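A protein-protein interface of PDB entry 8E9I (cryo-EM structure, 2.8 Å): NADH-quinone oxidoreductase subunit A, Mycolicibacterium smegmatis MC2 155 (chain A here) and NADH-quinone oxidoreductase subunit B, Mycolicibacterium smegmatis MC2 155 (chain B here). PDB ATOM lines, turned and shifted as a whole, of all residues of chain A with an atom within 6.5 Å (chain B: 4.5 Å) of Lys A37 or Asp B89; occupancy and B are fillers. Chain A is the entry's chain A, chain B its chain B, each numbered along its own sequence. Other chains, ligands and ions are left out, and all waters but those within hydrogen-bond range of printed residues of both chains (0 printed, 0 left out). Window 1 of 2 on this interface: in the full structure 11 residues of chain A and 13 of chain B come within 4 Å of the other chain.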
ATOM      1  N   PRO A  30     -32.214 -14.306   7.497  1.00  0.00           N
ATOM      2  CA  PRO A  30     -31.791 -13.626   8.722  1.00  0.00           C
ATOM      3  C   PRO A  30     -31.666 -12.129   8.510  1.00  0.00           C
ATOM      4  O   PRO A  30     -31.480 -11.640   7.396  1.00  0.00           O
ATOM      5  CB  PRO A  30     -30.427 -14.257   9.027  1.00  0.00           C
ATOM      6  CG  PRO A  30     -30.411 -15.530   8.267  1.00  0.00           C
ATOM      7  CD  PRO A  30     -31.205 -15.269   7.035  1.00  0.00           C
ATOM      8  N   ARG A  31     -31.804 -11.394   9.603  1.00  0.00           N
ATOM      9  CA  ARG A  31     -31.513  -9.973   9.629  1.00  0.00           C
ATOM     10  C   ARG A  31     -30.908  -9.621  10.975  1.00  0.00           C
ATOM     11  O   ARG A  31     -31.521  -9.856  12.019  1.00  0.00           O
ATOM     12  CB  ARG A  31     -32.763  -9.133   9.386  1.00  0.00           C
ATOM     13  CG  ARG A  31     -33.368  -9.322   8.017  1.00  0.00           C
ATOM     14  CD  ARG A  31     -34.130  -8.086   7.605  1.00  0.00           C
ATOM     15  NE  ARG A  31     -33.242  -7.078   7.039  1.00  0.00           N
ATOM     16  CZ  ARG A  31     -32.913  -5.938   7.636  1.00  0.00           C
ATOM     17  NH1 ARG A  31     -33.401  -5.606   8.822  1.00  0.00           N
ATOM     18  NH2 ARG A  31     -32.071  -5.110   7.028  1.00  0.00           N
ATOM     19  N   ARG A  32     -29.707  -9.055  10.943  1.00  0.00           N
ATOM     20  CA  ARG A  32     -29.037  -8.630  12.167  1.00  0.00           C
ATOM     21  C   ARG A  32     -28.289  -7.339  11.874  1.00  0.00           C
ATOM     22  O   ARG A  32     -27.463  -7.291  10.960  1.00  0.00           O
ATOM     23  CB  ARG A  32     -28.087  -9.702  12.683  1.00  0.00           C
ATOM     24  CG  ARG A  32     -27.386  -9.280  13.951  1.00  0.00           C
ATOM     25  CD  ARG A  32     -26.659 -10.413  14.619  1.00  0.00           C
ATOM     26  NE  ARG A  32     -26.057  -9.961  15.867  1.00  0.00           N
ATOM     27  CZ  ARG A  32     -26.744  -9.693  16.968  1.00  0.00           C
ATOM     28  NH1 ARG A  32     -28.056  -9.853  17.021  1.00  0.00           N
ATOM     29  NH2 ARG A  32     -26.100  -9.246  18.040  1.00  0.00           N
ATOM     30  N   PHE A  33     -28.577  -6.301  12.650  1.00  0.00           N
ATOM     31  CA  PHE A  33     -27.888  -5.036  12.468  1.00  0.00           C
ATOM     32  C   PHE A  33     -26.418  -5.171  12.835  1.00  0.00           C
ATOM     33  O   PHE A  33     -26.062  -5.790  13.839  1.00  0.00           O
ATOM     34  CB  PHE A  33     -28.543  -3.949  13.316  1.00  0.00           C
ATOM     35  CG  PHE A  33     -27.748  -2.686  13.385  1.00  0.00           C
ATOM     36  CD1 PHE A  33     -27.849  -1.735  12.392  1.00  0.00           C
ATOM     37  CD2 PHE A  33     -26.894  -2.453  14.443  1.00  0.00           C
ATOM     38  CE1 PHE A  33     -27.112  -0.573  12.454  1.00  0.00           C
ATOM     39  CE2 PHE A  33     -26.160  -1.297  14.510  1.00  0.00           C
ATOM     40  CZ  PHE A  33     -26.267  -0.356  13.513  1.00  0.00           C
ATOM     41  N   ASN A  34     -25.559  -4.584  12.011  1.00  0.00           N
ATOM     42  CA  ASN A  34     -24.132  -4.545  12.305  1.00  0.00           C
ATOM     43  C   ASN A  34     -23.539  -3.369  11.557  1.00  0.00           C
ATOM     44  O   ASN A  34     -23.640  -3.306  10.330  1.00  0.00           O
ATOM     45  CB  ASN A  34     -23.448  -5.840  11.899  1.00  0.00           C
ATOM     46  CG  ASN A  34     -21.967  -5.833  12.208  1.00  0.00           C
ATOM     47  OD1 ASN A  34     -21.243  -4.923  11.809  1.00  0.00           O
ATOM     48  ND2 ASN A  34     -21.505  -6.857  12.915  1.00  0.00           N
ATOM     49  N   ARG A  35     -22.915  -2.448  12.284  1.00  0.00           N
ATOM     50  CA  ARG A  35     -22.382  -1.259  11.637  1.00  0.00           C
ATOM     51  C   ARG A  35     -21.355  -1.636  10.578  1.00  0.00           C
ATOM     52  O   ARG A  35     -21.326  -1.046   9.494  1.00  0.00           O
ATOM     53  CB  ARG A  35     -21.774  -0.333  12.685  1.00  0.00           C
ATOM     54  CG  ARG A  35     -22.821   0.230  13.619  1.00  0.00           C
ATOM     55  CD  ARG A  35     -22.218   0.961  14.802  1.00  0.00           C
ATOM     56  NE  ARG A  35     -23.257   1.616  15.586  1.00  0.00           N
ATOM     57  CZ  ARG A  35     -24.073   0.979  16.416  1.00  0.00           C
ATOM     58  NH1 ARG A  35     -23.959  -0.318  16.637  1.00  0.00           N
ATOM     59  NH2 ARG A  35     -25.020   1.665  17.049  1.00  0.00           N
ATOM     60  N   SER A  36     -20.507  -2.622  10.872  1.00  0.00           N
ATOM     61  CA  SER A  36     -19.526  -3.074   9.891  1.00  0.00           C
ATOM     62  C   SER A  36     -20.208  -3.662   8.663  1.00  0.00           C
ATOM     63  O   SER A  36     -19.809  -3.391   7.527  1.00  0.00           O
ATOM     64  CB  SER A  36     -18.588  -4.098  10.528  1.00  0.00           C
ATOM     65  OG  SER A  36     -17.543  -4.452   9.643  1.00  0.00           O
ATOM     66  N   LYS A  37     -21.246  -4.469   8.874  1.00  0.00           N
ATOM     67  CA  LYS A  37     -21.944  -5.070   7.744  1.00  0.00           C
ATOM     68  C   LYS A  37     -22.563  -4.007   6.855  1.00  0.00           C
ATOM     69  O   LYS A  37     -22.549  -4.125   5.626  1.00  0.00           O
ATOM     70  CB  LYS A  37     -23.021  -6.026   8.242  1.00  0.00           C
ATOM     71  CG  LYS A  37     -23.721  -6.779   7.136  1.00  0.00           C
ATOM     72  CD  LYS A  37     -24.953  -7.502   7.643  1.00  0.00           C
ATOM     73  CE  LYS A  37     -24.586  -8.614   8.603  1.00  0.00           C
ATOM     74  NZ  LYS A  37     -25.790  -9.276   9.159  1.00  0.00           N
ATOM     75  N   LEU A  38     -23.125  -2.968   7.459  1.00  0.00           N
ATOM     76  CA  LEU A  38     -23.832  -1.938   6.720  1.00  0.00           C
ATOM     77  C   LEU A  38     -22.907  -0.879   6.137  1.00  0.00           C
ATOM     78  O   LEU A  38     -23.366  -0.043   5.355  1.00  0.00           O
ATOM     79  CB  LEU A  38     -24.863  -1.269   7.629  1.00  0.00           C
ATOM     80  CG  LEU A  38     -25.853  -2.228   8.286  1.00  0.00           C
ATOM     81  CD1 LEU A  38     -26.805  -1.462   9.172  1.00  0.00           C
ATOM     82  CD2 LEU A  38     -26.616  -3.041   7.257  1.00  0.00           C
ATOM     83  N   GLU A  39     -21.630  -0.887   6.495  1.00  0.00           N
ATOM     84  CA  GLU A  39     -20.698   0.070   5.931  1.00  0.00           C
ATOM     85  C   GLU A  39     -20.388  -0.288   4.480  1.00  0.00           C
ATOM     86  O   GLU A  39     -20.549  -1.429   4.041  1.00  0.00           O
ATOM     87  CB  GLU A  39     -19.414   0.118   6.758  1.00  0.00           C
ATOM     88  N   ALA A  40     -19.933   0.708   3.730  1.00  0.00           N
ATOM     89  CA  ALA A  40     -19.611   0.489   2.330  1.00  0.00           C
ATOM     90  C   ALA A  40     -18.537  -0.578   2.202  1.00  0.00           C
ATOM     91  O   ALA A  40     -17.680  -0.736   3.074  1.00  0.00           O
ATOM     92  CB  ALA A  40     -19.133   1.789   1.684  1.00  0.00           C
ATOM     93  N   ARG B  65     -20.838  -9.419  -0.217  1.00  0.00           N
ATOM     94  CA  ARG B  65     -22.288  -9.465  -0.076  1.00  0.00           C
ATOM     95  C   ARG B  65     -22.857 -10.770  -0.616  1.00  0.00           C
ATOM     96  O   ARG B  65     -23.677 -11.416   0.045  1.00  0.00           O
ATOM     97  CB  ARG B  65     -22.925  -8.273  -0.786  1.00  0.00           C
ATOM     98  CG  ARG B  65     -22.267  -6.944  -0.495  1.00  0.00           C
ATOM     99  CD  ARG B  65     -22.074  -6.731   0.988  1.00  0.00           C
ATOM    100  NE  ARG B  65     -21.776  -5.340   1.310  1.00  0.00           N
ATOM    101  CZ  ARG B  65     -21.864  -4.818   2.524  1.00  0.00           C
ATOM    102  NH1 ARG B  65     -22.242  -5.546   3.562  1.00  0.00           N
ATOM    103  NH2 ARG B  65     -21.564  -3.538   2.704  1.00  0.00           N
ATOM    104  N   ARG B  85     -11.733  -9.655   9.325  1.00  0.00           N
ATOM    105  CA  ARG B  85     -12.959  -9.454  10.086  1.00  0.00           C
ATOM    106  C   ARG B  85     -13.915  -8.531   9.351  1.00  0.00           C
ATOM    107  O   ARG B  85     -15.128  -8.748   9.366  1.00  0.00           O
ATOM    108  CB  ARG B  85     -12.633  -8.890  11.463  1.00  0.00           C
ATOM    109  CG  ARG B  85     -13.849  -8.612  12.323  1.00  0.00           C
ATOM    110  CD  ARG B  85     -14.428  -9.871  12.903  1.00  0.00           C
ATOM    111  NE  ARG B  85     -15.879  -9.799  12.988  1.00  0.00           N
ATOM    112  CZ  ARG B  85     -16.630 -10.643  13.675  1.00  0.00           C
ATOM    113  NH1 ARG B  85     -16.096 -11.629  14.375  1.00  0.00           N
ATOM    114  NH2 ARG B  85     -17.949 -10.495  13.662  1.00  0.00           N
ATOM    115  N   GLN B  86     -13.396  -7.476   8.726  1.00  0.00           N
ATOM    116  CA  GLN B  86     -14.268  -6.585   7.975  1.00  0.00           C
ATOM    117  C   GLN B  86     -14.964  -7.335   6.855  1.00  0.00           C
ATOM    118  O   GLN B  86     -16.174  -7.189   6.655  1.00  0.00           O
ATOM    119  CB  GLN B  86     -13.469  -5.412   7.414  1.00  0.00           C
ATOM    120  CG  GLN B  86     -14.318  -4.384   6.699  1.00  0.00           C
ATOM    121  CD  GLN B  86     -15.219  -3.632   7.641  1.00  0.00           C
ATOM    122  OE1 GLN B  86     -15.156  -3.816   8.855  1.00  0.00           O
ATOM    123  NE2 GLN B  86     -16.070  -2.783   7.090  1.00  0.00           N
ATOM    124  N   ILE B  87     -14.220  -8.157   6.121  1.00  0.00           N
ATOM    125  CA  ILE B  87     -14.828  -8.928   5.044  1.00  0.00           C
ATOM    126  C   ILE B  87     -15.877  -9.874   5.603  1.00  0.00           C
ATOM    127  O   ILE B  87     -16.973 -10.009   5.050  1.00  0.00           O
ATOM    128  CB  ILE B  87     -13.756  -9.691   4.250  1.00  0.00           C
ATOM    129  CG1 ILE B  87     -12.778  -8.715   3.601  1.00  0.00           C
ATOM    130  CG2 ILE B  87     -14.414 -10.569   3.205  1.00  0.00           C
ATOM    131  CD1 ILE B  87     -13.419  -7.724   2.667  1.00  0.00           C
ATOM    132  N   TYR B  88     -15.557 -10.550   6.707  1.00  0.00           N
ATOM    133  CA  TYR B  88     -16.530 -11.454   7.304  1.00  0.00           C
ATOM    134  C   TYR B  88     -17.805 -10.714   7.671  1.00  0.00           C
ATOM    135  O   TYR B  88     -18.905 -11.119   7.282  1.00  0.00           O
ATOM    136  CB  TYR B  88     -15.950 -12.126   8.542  1.00  0.00           C
ATOM    137  CG  TYR B  88     -16.970 -12.945   9.296  1.00  0.00           C
ATOM    138  CD1 TYR B  88     -17.358 -14.193   8.841  1.00  0.00           C
ATOM    139  CD2 TYR B  88     -17.562 -12.459  10.448  1.00  0.00           C
ATOM    140  CE1 TYR B  88     -18.286 -14.939   9.523  1.00  0.00           C
ATOM    141  CE2 TYR B  88     -18.499 -13.201  11.134  1.00  0.00           C
ATOM    142  CZ  TYR B  88     -18.853 -14.439  10.666  1.00  0.00           C
ATOM    143  OH  TYR B  88     -19.785 -15.185  11.343  1.00  0.00           O
ATOM    144  N   ASP B  89     -17.671  -9.617   8.413  1.00  0.00           N
ATOM    145  CA  ASP B  89     -18.837  -8.860   8.843  1.00  0.00           C
ATOM    146  C   ASP B  89     -19.599  -8.299   7.657  1.00  0.00           C
ATOM    147  O   ASP B  89     -20.800  -8.033   7.764  1.00  0.00           O
ATOM    148  CB  ASP B  89     -18.405  -7.734   9.781  1.00  0.00           C
ATOM    149  N   GLN B  90     -18.930  -8.106   6.525  1.00  0.00           N
ATOM    150  CA  GLN B  90     -19.608  -7.578   5.353  1.00  0.00           C
ATOM    151  C   GLN B  90     -20.283  -8.648   4.507  1.00  0.00           C
ATOM    152  O   GLN B  90     -20.979  -8.293   3.554  1.00  0.00           O
ATOM    153  CB  GLN B  90     -18.634  -6.780   4.493  1.00  0.00           C
ATOM    154  CG  GLN B  90     -18.292  -5.437   5.094  1.00  0.00           C
ATOM    155  CD  GLN B  90     -17.607  -4.521   4.113  1.00  0.00           C
ATOM    156  OE1 GLN B  90     -17.072  -4.966   3.103  1.00  0.00           O
ATOM    157  NE2 GLN B  90     -17.625  -3.229   4.402  1.00  0.00           N
ATOM    158  N   MET B  91     -20.101  -9.934   4.799  1.00  0.00           N
ATOM    159  CA  MET B  91     -21.003 -10.922   4.227  1.00  0.00           C
ATOM    160  C   MET B  91     -22.352 -10.818   4.912  1.00  0.00           C
ATOM    161  O   MET B  91     -22.439 -10.406   6.071  1.00  0.00           O
ATOM    162  CB  MET B  91     -20.477 -12.349   4.362  1.00  0.00           C
ATOM    163  CG  MET B  91     -19.454 -12.755   3.324  1.00  0.00           C
ATOM    164  SD  MET B  91     -18.632 -14.294   3.730  1.00  0.00           S
ATOM    165  CE  MET B  91     -17.665 -13.762   5.102  1.00  0.00           C
ATOM    166  N   GLU B  93     -25.734 -12.603   6.412  1.00  0.00           N
ATOM    167  CA  GLU B  93     -26.061 -13.880   7.006  1.00  0.00           C
ATOM    168  C   GLU B  93     -27.075 -14.619   6.140  1.00  0.00           C
ATOM    169  O   GLU B  93     -27.792 -14.007   5.350  1.00  0.00           O
ATOM    170  CB  GLU B  93     -26.619 -13.683   8.412  1.00  0.00           C
ATOM    171  N   LYS B  95     -23.847 -17.078   7.194  1.00  0.00           N
ATOM    172  CA  LYS B  95     -22.508 -17.200   6.648  1.00  0.00           C
ATOM    173  C   LYS B  95     -21.713 -18.147   7.526  1.00  0.00           C
ATOM    174  O   LYS B  95     -21.842 -18.134   8.753  1.00  0.00           O
ATOM    175  CB  LYS B  95     -21.810 -15.841   6.564  1.00  0.00           C
ATOM    176  CG  LYS B  95     -21.806 -15.075   7.870  1.00  0.00           C
ATOM    177  CD  LYS B  95     -21.355 -13.642   7.684  1.00  0.00           C
ATOM    178  CE  LYS B  95     -21.633 -12.812   8.920  1.00  0.00           C
ATOM    179  NZ  LYS B  95     -21.359 -11.370   8.702  1.00  0.00           N
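The guanidinium group (NH1) of Arg B65 is in hydrogen-bond range of the backbone carbonyl oxygen (O) of Lys A37 (2.5 Å).
O of Glu A39 lies within hydrogen-bond range of NH2 of Arg B65.
OE1 of Gln B86 is in hydrogen-bond range of OG of Ser A36.
NE2 of Gln B90 lies within hydrogen-bond range of O of Glu A39 (3.5 Å).
NE2 of Gln B90 sits at hydrogen-bond distance from O of Ala A40 (2.8 Å).
The guanidinium group of Arg B65 lies within hydrogen-bond range of the backbone carbonyl oxygen of Gln B90 (3.0 Å).
NE2 of Gln B86 lies close to NE2 of Gln B90 (3.1 Å).
O of Met B91 is in hydrogen-bond range of NZ of Lys B95.
The side-chain amino group of Lys A37 sits at hydrogen-bond distance from the backbone carbonyl oxygen of Arg A32 (3.2 Å).
The backbone NH of Ser A36 sits at hydrogen-bond distance from the side-chain amide oxygen of Asn A34, 2.6 Å away.
OD1 of Asn A34 sits at hydrogen-bond distance from N of Lys A37.
Hydrophobic or aromatic side chains of chain A that line the printed part of chain B: Pro A30.
Along chain A the printed residues that touch a printed residue of chain B span positions 30 to 40.
Among the printed residues, 10 pairs touch across the chains.
Among the printed residues, no Asp or Glu carboxylate lies within 4 Å of a Lys or Arg side-chain nitrogen of the other chain.
Pro A30 touches Glu B93.
OG of Ser A36 touches CB of Asp B89 (3.4 Å).
O of Ser A36 touches CG of Gln B90, at 3.5 Å.
O of Asp B89 touches CB of Lys A37, at 3.0 Å.
O of Met B91 touches CE of Lys A37 (3.8 Å).
Lys A37 touches just these residues of chain B: Arg B65 (2.5 Å), Asp B89 (3.0 Å) and Met B91 (3.8 Å).
Of chain A, only Ser A36 and Lys A37 come within 4 Å of Asp B89.
Of the printed residues of chain A, Glu B93 touches Pro A30.
Printed residues of chain B within 4 Å of Ala A40: Gln B90 (2.8 Å).
Printed residues of chain A within 4 Å of Gln B86: Ser A36.
Of the printed residues of chain A, Met B91 touches Lys A37 (3.8 Å).
Printed residues of chain B within 4 Å of Glu A39: Arg B65 and Gln B90.
Arg A31 touches none of the printed residues of chain B.
The nearest residue of chain A that does not touch Asp B89 is Asn A34 (4.5 Å).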
